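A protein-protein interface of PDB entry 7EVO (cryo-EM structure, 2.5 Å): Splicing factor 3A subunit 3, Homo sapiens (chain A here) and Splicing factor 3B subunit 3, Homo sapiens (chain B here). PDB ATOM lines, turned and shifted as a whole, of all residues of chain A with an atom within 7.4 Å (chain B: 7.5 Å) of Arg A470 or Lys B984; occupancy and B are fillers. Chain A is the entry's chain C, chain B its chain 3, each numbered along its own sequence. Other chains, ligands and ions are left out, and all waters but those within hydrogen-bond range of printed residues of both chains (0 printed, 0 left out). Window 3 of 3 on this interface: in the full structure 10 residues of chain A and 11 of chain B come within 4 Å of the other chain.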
ATOM      1  N   LYS A 463     -16.123 -19.007  11.108  1.00  0.00           N
ATOM      2  CA  LYS A 463     -14.729 -18.633  11.297  1.00  0.00           C
ATOM      3  C   LYS A 463     -13.932 -19.786  11.888  1.00  0.00           C
ATOM      4  O   LYS A 463     -12.864 -20.141  11.379  1.00  0.00           O
ATOM      5  CB  LYS A 463     -14.638 -17.397  12.192  1.00  0.00           C
ATOM      6  CG  LYS A 463     -13.871 -16.238  11.580  1.00  0.00           C
ATOM      7  CD  LYS A 463     -14.172 -14.939  12.307  1.00  0.00           C
ATOM      8  CE  LYS A 463     -13.105 -13.895  12.029  1.00  0.00           C
ATOM      9  NZ  LYS A 463     -13.063 -12.853  13.091  1.00  0.00           N
ATOM     10  N   LEU A 464     -14.429 -20.374  12.981  1.00  0.00           N
ATOM     11  CA  LEU A 464     -13.725 -21.500  13.587  1.00  0.00           C
ATOM     12  C   LEU A 464     -13.542 -22.638  12.589  1.00  0.00           C
ATOM     13  O   LEU A 464     -12.431 -23.158  12.430  1.00  0.00           O
ATOM     14  CB  LEU A 464     -14.474 -21.985  14.826  1.00  0.00           C
ATOM     15  CG  LEU A 464     -13.789 -23.081  15.648  1.00  0.00           C
ATOM     16  CD1 LEU A 464     -13.863 -22.768  17.134  1.00  0.00           C
ATOM     17  CD2 LEU A 464     -14.406 -24.442  15.356  1.00  0.00           C
ATOM     18  N   GLN A 465     -14.615 -23.011  11.883  1.00  0.00           N
ATOM     19  CA  GLN A 465     -14.538 -24.086  10.895  1.00  0.00           C
ATOM     20  C   GLN A 465     -13.484 -23.817   9.827  1.00  0.00           C
ATOM     21  O   GLN A 465     -12.571 -24.636   9.629  1.00  0.00           O
ATOM     22  CB  GLN A 465     -15.901 -24.270  10.228  1.00  0.00           C
ATOM     23  CG  GLN A 465     -16.103 -25.616   9.561  1.00  0.00           C
ATOM     24  CD  GLN A 465     -17.274 -25.610   8.600  1.00  0.00           C
ATOM     25  OE1 GLN A 465     -17.112 -25.855   7.405  1.00  0.00           O
ATOM     26  NE2 GLN A 465     -18.463 -25.325   9.117  1.00  0.00           N
ATOM     27  N   LYS A 466     -13.587 -22.682   9.132  1.00  0.00           N
ATOM     28  CA  LYS A 466     -12.661 -22.406   8.040  1.00  0.00           C
ATOM     29  C   LYS A 466     -11.232 -22.272   8.547  1.00  0.00           C
ATOM     30  O   LYS A 466     -10.317 -22.895   7.996  1.00  0.00           O
ATOM     31  CB  LYS A 466     -13.095 -21.155   7.276  1.00  0.00           C
ATOM     32  CG  LYS A 466     -13.808 -21.474   5.970  1.00  0.00           C
ATOM     33  CD  LYS A 466     -14.357 -20.229   5.291  1.00  0.00           C
ATOM     34  CE  LYS A 466     -15.312 -19.463   6.193  1.00  0.00           C
ATOM     35  NZ  LYS A 466     -15.504 -18.062   5.720  1.00  0.00           N
ATOM     36  N   ALA A 467     -11.017 -21.480   9.603  1.00  0.00           N
ATOM     37  CA  ALA A 467      -9.673 -21.321  10.149  1.00  0.00           C
ATOM     38  C   ALA A 467      -9.079 -22.665  10.548  1.00  0.00           C
ATOM     39  O   ALA A 467      -7.869 -22.884  10.416  1.00  0.00           O
ATOM     40  CB  ALA A 467      -9.700 -20.365  11.342  1.00  0.00           C
ATOM     41  N   SER A 468      -9.918 -23.585  11.031  1.00  0.00           N
ATOM     42  CA  SER A 468      -9.434 -24.921  11.356  1.00  0.00           C
ATOM     43  C   SER A 468      -9.011 -25.679  10.106  1.00  0.00           C
ATOM     44  O   SER A 468      -7.970 -26.346  10.101  1.00  0.00           O
ATOM     45  CB  SER A 468     -10.513 -25.695  12.110  1.00  0.00           C
ATOM     46  OG  SER A 468     -10.457 -27.077  11.802  1.00  0.00           O
ATOM     47  N   GLU A 469      -9.801 -25.593   9.033  1.00  0.00           N
ATOM     48  CA  GLU A 469      -9.591 -26.524   7.927  1.00  0.00           C
ATOM     49  C   GLU A 469      -8.500 -26.042   6.968  1.00  0.00           C
ATOM     50  O   GLU A 469      -8.127 -26.762   6.035  1.00  0.00           O
ATOM     51  CB  GLU A 469     -10.913 -26.774   7.197  1.00  0.00           C
ATOM     52  CG  GLU A 469     -10.859 -27.894   6.165  1.00  0.00           C
ATOM     53  CD  GLU A 469     -12.227 -28.420   5.784  1.00  0.00           C
ATOM     54  OE1 GLU A 469     -12.320 -29.613   5.424  1.00  0.00           O
ATOM     55  OE2 GLU A 469     -13.206 -27.648   5.848  1.00  0.00           O
ATOM     56  N   ARG A 470      -7.952 -24.847   7.186  1.00  0.00           N
ATOM     57  CA  ARG A 470      -6.843 -24.409   6.344  1.00  0.00           C
ATOM     58  C   ARG A 470      -5.535 -25.073   6.759  1.00  0.00           C
ATOM     59  O   ARG A 470      -5.452 -25.766   7.776  1.00  0.00           O
ATOM     60  CB  ARG A 470      -6.649 -22.891   6.386  1.00  0.00           C
ATOM     61  CG  ARG A 470      -7.890 -22.037   6.362  1.00  0.00           C
ATOM     62  CD  ARG A 470      -7.699 -20.837   7.275  1.00  0.00           C
ATOM     63  NE  ARG A 470      -8.661 -19.771   7.019  1.00  0.00           N
ATOM     64  CZ  ARG A 470      -8.456 -18.770   6.170  1.00  0.00           C
ATOM     65  NH1 ARG A 470      -7.318 -18.692   5.493  1.00  0.00           N
ATOM     66  NH2 ARG A 470      -9.387 -17.841   6.002  1.00  0.00           N
ATOM     67  N   TRP A 471      -4.504 -24.849   5.948  1.00  0.00           N
ATOM     68  CA  TRP A 471      -3.143 -25.280   6.245  1.00  0.00           C
ATOM     69  C   TRP A 471      -2.339 -24.070   6.705  1.00  0.00           C
ATOM     70  O   TRP A 471      -1.987 -23.209   5.891  1.00  0.00           O
ATOM     71  CB  TRP A 471      -2.497 -25.924   5.017  1.00  0.00           C
ATOM     72  CG  TRP A 471      -0.992 -25.957   5.055  1.00  0.00           C
ATOM     73  CD1 TRP A 471      -0.139 -25.270   4.241  1.00  0.00           C
ATOM     74  CD2 TRP A 471      -0.169 -26.731   5.934  1.00  0.00           C
ATOM     75  NE1 TRP A 471       1.162 -25.560   4.566  1.00  0.00           N
ATOM     76  CE2 TRP A 471       1.172 -26.452   5.604  1.00  0.00           C
ATOM     77  CE3 TRP A 471      -0.434 -27.624   6.975  1.00  0.00           C
ATOM     78  CZ2 TRP A 471       2.241 -27.036   6.274  1.00  0.00           C
ATOM     79  CZ3 TRP A 471       0.631 -28.205   7.637  1.00  0.00           C
ATOM     80  CH2 TRP A 471       1.952 -27.911   7.282  1.00  0.00           C
ATOM     81  N   GLN A 472      -2.058 -24.000   8.003  1.00  0.00           N
ATOM     82  CA  GLN A 472      -1.303 -22.885   8.564  1.00  0.00           C
ATOM     83  C   GLN A 472       0.127 -23.322   8.847  1.00  0.00           C
ATOM     84  O   GLN A 472       0.384 -23.937   9.893  1.00  0.00           O
ATOM     85  CB  GLN A 472      -1.968 -22.363   9.838  1.00  0.00           C
ATOM     86  CG  GLN A 472      -2.739 -23.411  10.620  1.00  0.00           C
ATOM     87  CD  GLN A 472      -4.238 -23.237  10.494  1.00  0.00           C
ATOM     88  OE1 GLN A 472      -4.747 -22.116  10.498  1.00  0.00           O
ATOM     89  NE2 GLN A 472      -4.957 -24.348  10.385  1.00  0.00           N
ATOM     90  N   PRO A 473       1.083 -23.015   7.968  1.00  0.00           N
ATOM     91  CA  PRO A 473       2.441 -23.556   8.147  1.00  0.00           C
ATOM     92  C   PRO A 473       3.164 -23.031   9.376  1.00  0.00           C
ATOM     93  O   PRO A 473       4.060 -23.710   9.892  1.00  0.00           O
ATOM     94  CB  PRO A 473       3.148 -23.139   6.850  1.00  0.00           C
ATOM     95  CG  PRO A 473       2.398 -21.945   6.378  1.00  0.00           C
ATOM     96  CD  PRO A 473       0.970 -22.169   6.769  1.00  0.00           C
ATOM     97  N   GLU A 476       1.713 -25.169  12.222  1.00  0.00           N
ATOM     98  CA  GLU A 476       1.732 -26.539  11.730  1.00  0.00           C
ATOM     99  C   GLU A 476       2.953 -26.737  10.848  1.00  0.00           C
ATOM    100  O   GLU A 476       2.910 -26.442   9.651  1.00  0.00           O
ATOM    101  CB  GLU A 476       0.465 -26.860  10.942  1.00  0.00           C
ATOM    102  CG  GLU A 476      -0.627 -27.515  11.748  1.00  0.00           C
ATOM    103  CD  GLU A 476      -1.910 -27.645  10.961  1.00  0.00           C
ATOM    104  OE1 GLU A 476      -2.518 -26.605  10.633  1.00  0.00           O
ATOM    105  OE2 GLU A 476      -2.307 -28.787  10.656  1.00  0.00           O
ATOM    106  N   LYS B 965      -7.981 -39.526   6.466  1.00  0.00           N
ATOM    107  CA  LYS B 965      -8.537 -38.539   5.555  1.00  0.00           C
ATOM    108  C   LYS B 965      -7.527 -37.501   5.085  1.00  0.00           C
ATOM    109  O   LYS B 965      -7.846 -36.714   4.191  1.00  0.00           O
ATOM    110  CB  LYS B 965      -9.709 -37.818   6.238  1.00  0.00           C
ATOM    111  CG  LYS B 965     -10.750 -37.258   5.304  1.00  0.00           C
ATOM    112  CD  LYS B 965     -11.624 -36.247   6.020  1.00  0.00           C
ATOM    113  CE  LYS B 965     -12.461 -36.915   7.092  1.00  0.00           C
ATOM    114  NZ  LYS B 965     -13.358 -35.953   7.790  1.00  0.00           N
ATOM    115  N   LEU B 966      -6.322 -37.487   5.650  1.00  0.00           N
ATOM    116  CA  LEU B 966      -5.374 -36.389   5.490  1.00  0.00           C
ATOM    117  C   LEU B 966      -4.275 -36.809   4.520  1.00  0.00           C
ATOM    118  O   LEU B 966      -3.831 -37.959   4.537  1.00  0.00           O
ATOM    119  CB  LEU B 966      -4.783 -35.993   6.841  1.00  0.00           C
ATOM    120  CG  LEU B 966      -5.555 -35.079   7.801  1.00  0.00           C
ATOM    121  CD1 LEU B 966      -7.028 -35.420   7.884  1.00  0.00           C
ATOM    122  CD2 LEU B 966      -4.936 -35.169   9.179  1.00  0.00           C
ATOM    123  N   LEU B 967      -3.844 -35.878   3.675  1.00  0.00           N
ATOM    124  CA  LEU B 967      -2.697 -36.101   2.807  1.00  0.00           C
ATOM    125  C   LEU B 967      -1.537 -35.227   3.265  1.00  0.00           C
ATOM    126  O   LEU B 967      -1.664 -34.000   3.316  1.00  0.00           O
ATOM    127  CB  LEU B 967      -3.062 -35.786   1.358  1.00  0.00           C
ATOM    128  CG  LEU B 967      -1.972 -35.983   0.308  1.00  0.00           C
ATOM    129  CD1 LEU B 967      -1.722 -37.456   0.062  1.00  0.00           C
ATOM    130  CD2 LEU B 967      -2.352 -35.280  -0.979  1.00  0.00           C
ATOM    131  N   ARG B 968      -0.403 -35.846   3.589  1.00  0.00           N
ATOM    132  CA  ARG B 968       0.708 -35.118   4.182  1.00  0.00           C
ATOM    133  C   ARG B 968       1.993 -35.380   3.411  1.00  0.00           C
ATOM    134  O   ARG B 968       2.172 -36.427   2.784  1.00  0.00           O
ATOM    135  CB  ARG B 968       0.898 -35.501   5.656  1.00  0.00           C
ATOM    136  CG  ARG B 968      -0.173 -34.964   6.580  1.00  0.00           C
ATOM    137  CD  ARG B 968      -0.055 -35.583   7.954  1.00  0.00           C
ATOM    138  NE  ARG B 968      -0.949 -34.956   8.918  1.00  0.00           N
ATOM    139  CZ  ARG B 968      -1.156 -35.414  10.146  1.00  0.00           C
ATOM    140  NH1 ARG B 968      -0.531 -36.507  10.562  1.00  0.00           N
ATOM    141  NH2 ARG B 968      -1.986 -34.781  10.959  1.00  0.00           N
ATOM    142  N   ARG B 979       6.625 -33.327   9.408  1.00  0.00           N
ATOM    143  CA  ARG B 979       5.507 -32.917   8.567  1.00  0.00           C
ATOM    144  C   ARG B 979       5.831 -31.595   7.885  1.00  0.00           C
ATOM    145  O   ARG B 979       6.289 -30.649   8.534  1.00  0.00           O
ATOM    146  CB  ARG B 979       4.239 -32.797   9.405  1.00  0.00           C
ATOM    147  CG  ARG B 979       3.021 -32.366   8.614  1.00  0.00           C
ATOM    148  CD  ARG B 979       1.739 -32.757   9.319  1.00  0.00           C
ATOM    149  NE  ARG B 979       1.262 -31.721  10.228  1.00  0.00           N
ATOM    150  CZ  ARG B 979       1.313 -31.807  11.552  1.00  0.00           C
ATOM    151  NH1 ARG B 979       1.824 -32.886  12.129  1.00  0.00           N
ATOM    152  NH2 ARG B 979       0.852 -30.817  12.300  1.00  0.00           N
ATOM    153  N   GLU B 982       0.246 -30.252   4.075  1.00  0.00           N
ATOM    154  CA  GLU B 982      -0.956 -31.004   4.409  1.00  0.00           C
ATOM    155  C   GLU B 982      -2.152 -30.444   3.656  1.00  0.00           C
ATOM    156  O   GLU B 982      -2.327 -29.225   3.581  1.00  0.00           O
ATOM    157  CB  GLU B 982      -1.213 -30.964   5.919  1.00  0.00           C
ATOM    158  CG  GLU B 982      -2.530 -31.573   6.343  1.00  0.00           C
ATOM    159  CD  GLU B 982      -2.611 -31.791   7.838  1.00  0.00           C
ATOM    160  OE1 GLU B 982      -1.742 -31.269   8.565  1.00  0.00           O
ATOM    161  OE2 GLU B 982      -3.547 -32.477   8.291  1.00  0.00           O
ATOM    162  N   ASN B 983      -2.961 -31.338   3.099  1.00  0.00           N
ATOM    163  CA  ASN B 983      -4.273 -30.995   2.574  1.00  0.00           C
ATOM    164  C   ASN B 983      -5.344 -31.704   3.392  1.00  0.00           C
ATOM    165  O   ASN B 983      -5.202 -32.874   3.753  1.00  0.00           O
ATOM    166  CB  ASN B 983      -4.395 -31.383   1.100  1.00  0.00           C
ATOM    167  CG  ASN B 983      -5.630 -30.799   0.442  1.00  0.00           C
ATOM    168  OD1 ASN B 983      -5.617 -29.670  -0.043  1.00  0.00           O
ATOM    169  ND2 ASN B 983      -6.710 -31.566   0.432  1.00  0.00           N
ATOM    170  N   LYS B 984      -6.424 -30.981   3.685  1.00  0.00           N
ATOM    171  CA  LYS B 984      -7.476 -31.510   4.540  1.00  0.00           C
ATOM    172  C   LYS B 984      -8.847 -31.554   3.880  1.00  0.00           C
ATOM    173  O   LYS B 984      -9.851 -31.513   4.597  1.00  0.00           O
ATOM    174  CB  LYS B 984      -7.567 -30.691   5.837  1.00  0.00           C
ATOM    175  CG  LYS B 984      -6.220 -30.382   6.473  1.00  0.00           C
ATOM    176  CD  LYS B 984      -6.273 -29.109   7.295  1.00  0.00           C
ATOM    177  CE  LYS B 984      -5.187 -29.085   8.354  1.00  0.00           C
ATOM    178  NZ  LYS B 984      -5.601 -29.815   9.582  1.00  0.00           N
ATOM    179  N   HIS B 985      -8.928 -31.644   2.552  1.00  0.00           N
ATOM    180  CA  HIS B 985     -10.221 -31.564   1.882  1.00  0.00           C
ATOM    181  C   HIS B 985     -10.570 -32.836   1.121  1.00  0.00           C
ATOM    182  O   HIS B 985     -11.529 -32.830   0.345  1.00  0.00           O
ATOM    183  CB  HIS B 985     -10.239 -30.366   0.934  1.00  0.00           C
ATOM    184  CG  HIS B 985     -10.105 -29.048   1.629  1.00  0.00           C
ATOM    185  ND1 HIS B 985      -9.169 -28.105   1.265  1.00  0.00           N
ATOM    186  CD2 HIS B 985     -10.788 -28.516   2.670  1.00  0.00           C
ATOM    187  CE1 HIS B 985      -9.282 -27.049   2.049  1.00  0.00           C
ATOM    188  NE2 HIS B 985     -10.256 -27.274   2.912  1.00  0.00           N
ATOM    189  N   ILE B 986      -9.818 -33.917   1.319  1.00  0.00           N
ATOM    190  CA  ILE B 986     -10.169 -35.198   0.717  1.00  0.00           C
ATOM    191  C   ILE B 986     -11.339 -35.798   1.487  1.00  0.00           C
ATOM    192  O   ILE B 986     -11.426 -35.667   2.713  1.00  0.00           O
ATOM    193  CB  ILE B 986      -8.943 -36.124   0.693  1.00  0.00           C
ATOM    194  CG1 ILE B 986      -8.018 -35.717  -0.455  1.00  0.00           C
ATOM    195  CG2 ILE B 986      -9.345 -37.581   0.542  1.00  0.00           C
ATOM    196  CD1 ILE B 986      -6.592 -36.159  -0.280  1.00  0.00           C
ATOM    197  N   ALA B 987     -12.253 -36.446   0.764  1.00  0.00           N
ATOM    198  CA  ALA B 987     -13.585 -36.744   1.283  1.00  0.00           C
ATOM    199  C   ALA B 987     -13.614 -37.673   2.491  1.00  0.00           C
ATOM    200  O   ALA B 987     -13.935 -37.233   3.600  1.00  0.00           O
ATOM    201  CB  ALA B 987     -14.448 -37.342   0.170  1.00  0.00           C
ATOM    202  N   LEU B1021      -0.642 -27.984  -1.261  1.00  0.00           N
ATOM    203  CA  LEU B1021      -1.314 -29.064  -1.971  1.00  0.00           C
ATOM    204  C   LEU B1021      -2.733 -28.621  -2.297  1.00  0.00           C
ATOM    205  O   LEU B1021      -3.549 -28.438  -1.389  1.00  0.00           O
ATOM    206  CB  LEU B1021      -1.337 -30.344  -1.133  1.00  0.00           C
ATOM    207  CG  LEU B1021       0.006 -31.006  -0.820  1.00  0.00           C
ATOM    208  CD1 LEU B1021      -0.141 -32.011   0.310  1.00  0.00           C
ATOM    209  CD2 LEU B1021       0.579 -31.673  -2.054  1.00  0.00           C
ATOM    210  N   ILE B1023      -6.311 -29.118  -4.589  1.00  0.00           N
ATOM    211  CA  ILE B1023      -7.177 -29.983  -5.381  1.00  0.00           C
ATOM    212  C   ILE B1023      -7.678 -29.190  -6.580  1.00  0.00           C
ATOM    213  O   ILE B1023      -8.263 -28.114  -6.420  1.00  0.00           O
ATOM    214  CB  ILE B1023      -8.354 -30.504  -4.542  1.00  0.00           C
ATOM    215  CG1 ILE B1023      -7.861 -31.467  -3.460  1.00  0.00           C
ATOM    216  CG2 ILE B1023      -9.395 -31.164  -5.430  1.00  0.00           C
ATOM    217  CD1 ILE B1023      -8.926 -31.858  -2.467  1.00  0.00           C
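OE2 of Glu A476 is in salt-bridge range of NZ of Lys B984, 3.6 Å away. The backbone carbonyl oxygen (O) of Lys B984 sits close to the side-chain carboxylate (OE1) of Glu A469 (3.2 Å). The side-chain carboxylate (OE2) of Glu A476 lies close to the side-chain carboxylate (OE1) of Glu B982, at 3.3 Å.
O of Arg A470 sits at hydrogen-bond distance from NE2 of Gln A472 (3.0 Å). The side-chain amide nitrogen (NE2) of Gln A472 sits close to the side-chain carboxylate (OE1) of Glu A476, at 3.3 Å. The side-chain carboxylate (OE2) of Glu B982 is in salt-bridge range of the guanidinium group (NE) of Arg B968. The guanidinium group (NE) of Arg B979 is in salt-bridge range of the side-chain carboxylate (OE1) of Glu B982 (3.5 Å). NZ of Lys B984 is in salt-bridge range of OE2 of Glu B982 (3.6 Å). ND2 of Asn B983 lies close to N of His B985, at 3.1 Å.
Among the printed residues, pairs that only touch across the chains: Glu A469 with His B985 (3.3 Å), Arg A470 with Lys B984 (3.4 Å), Trp A471 with Glu B982 (3.6 Å) and Glu A476 with Arg B979 (3.7 Å).
Of chain B, only Lys B984 comes within 4 Å of Arg A470. Of the printed residues of chain B, Trp A471 touches Glu B982 (3.6 Å). Of the printed residues of chain A, Glu B982 touches Trp A471 and Glu A476. Lys B965 touches none of the printed residues of chain A. Asn B983 touches none of the printed residues of chain A. The nearest printed residue of chain B that does not touch Trp A471 is Arg B979 (4.4 Å).
Printed residues of chain A that touch a printed residue of chain B: Glu A469, Arg A470, Trp A471 and Glu A476. Along chain A the printed residues that touch a printed residue of chain B span positions 469 to 476.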
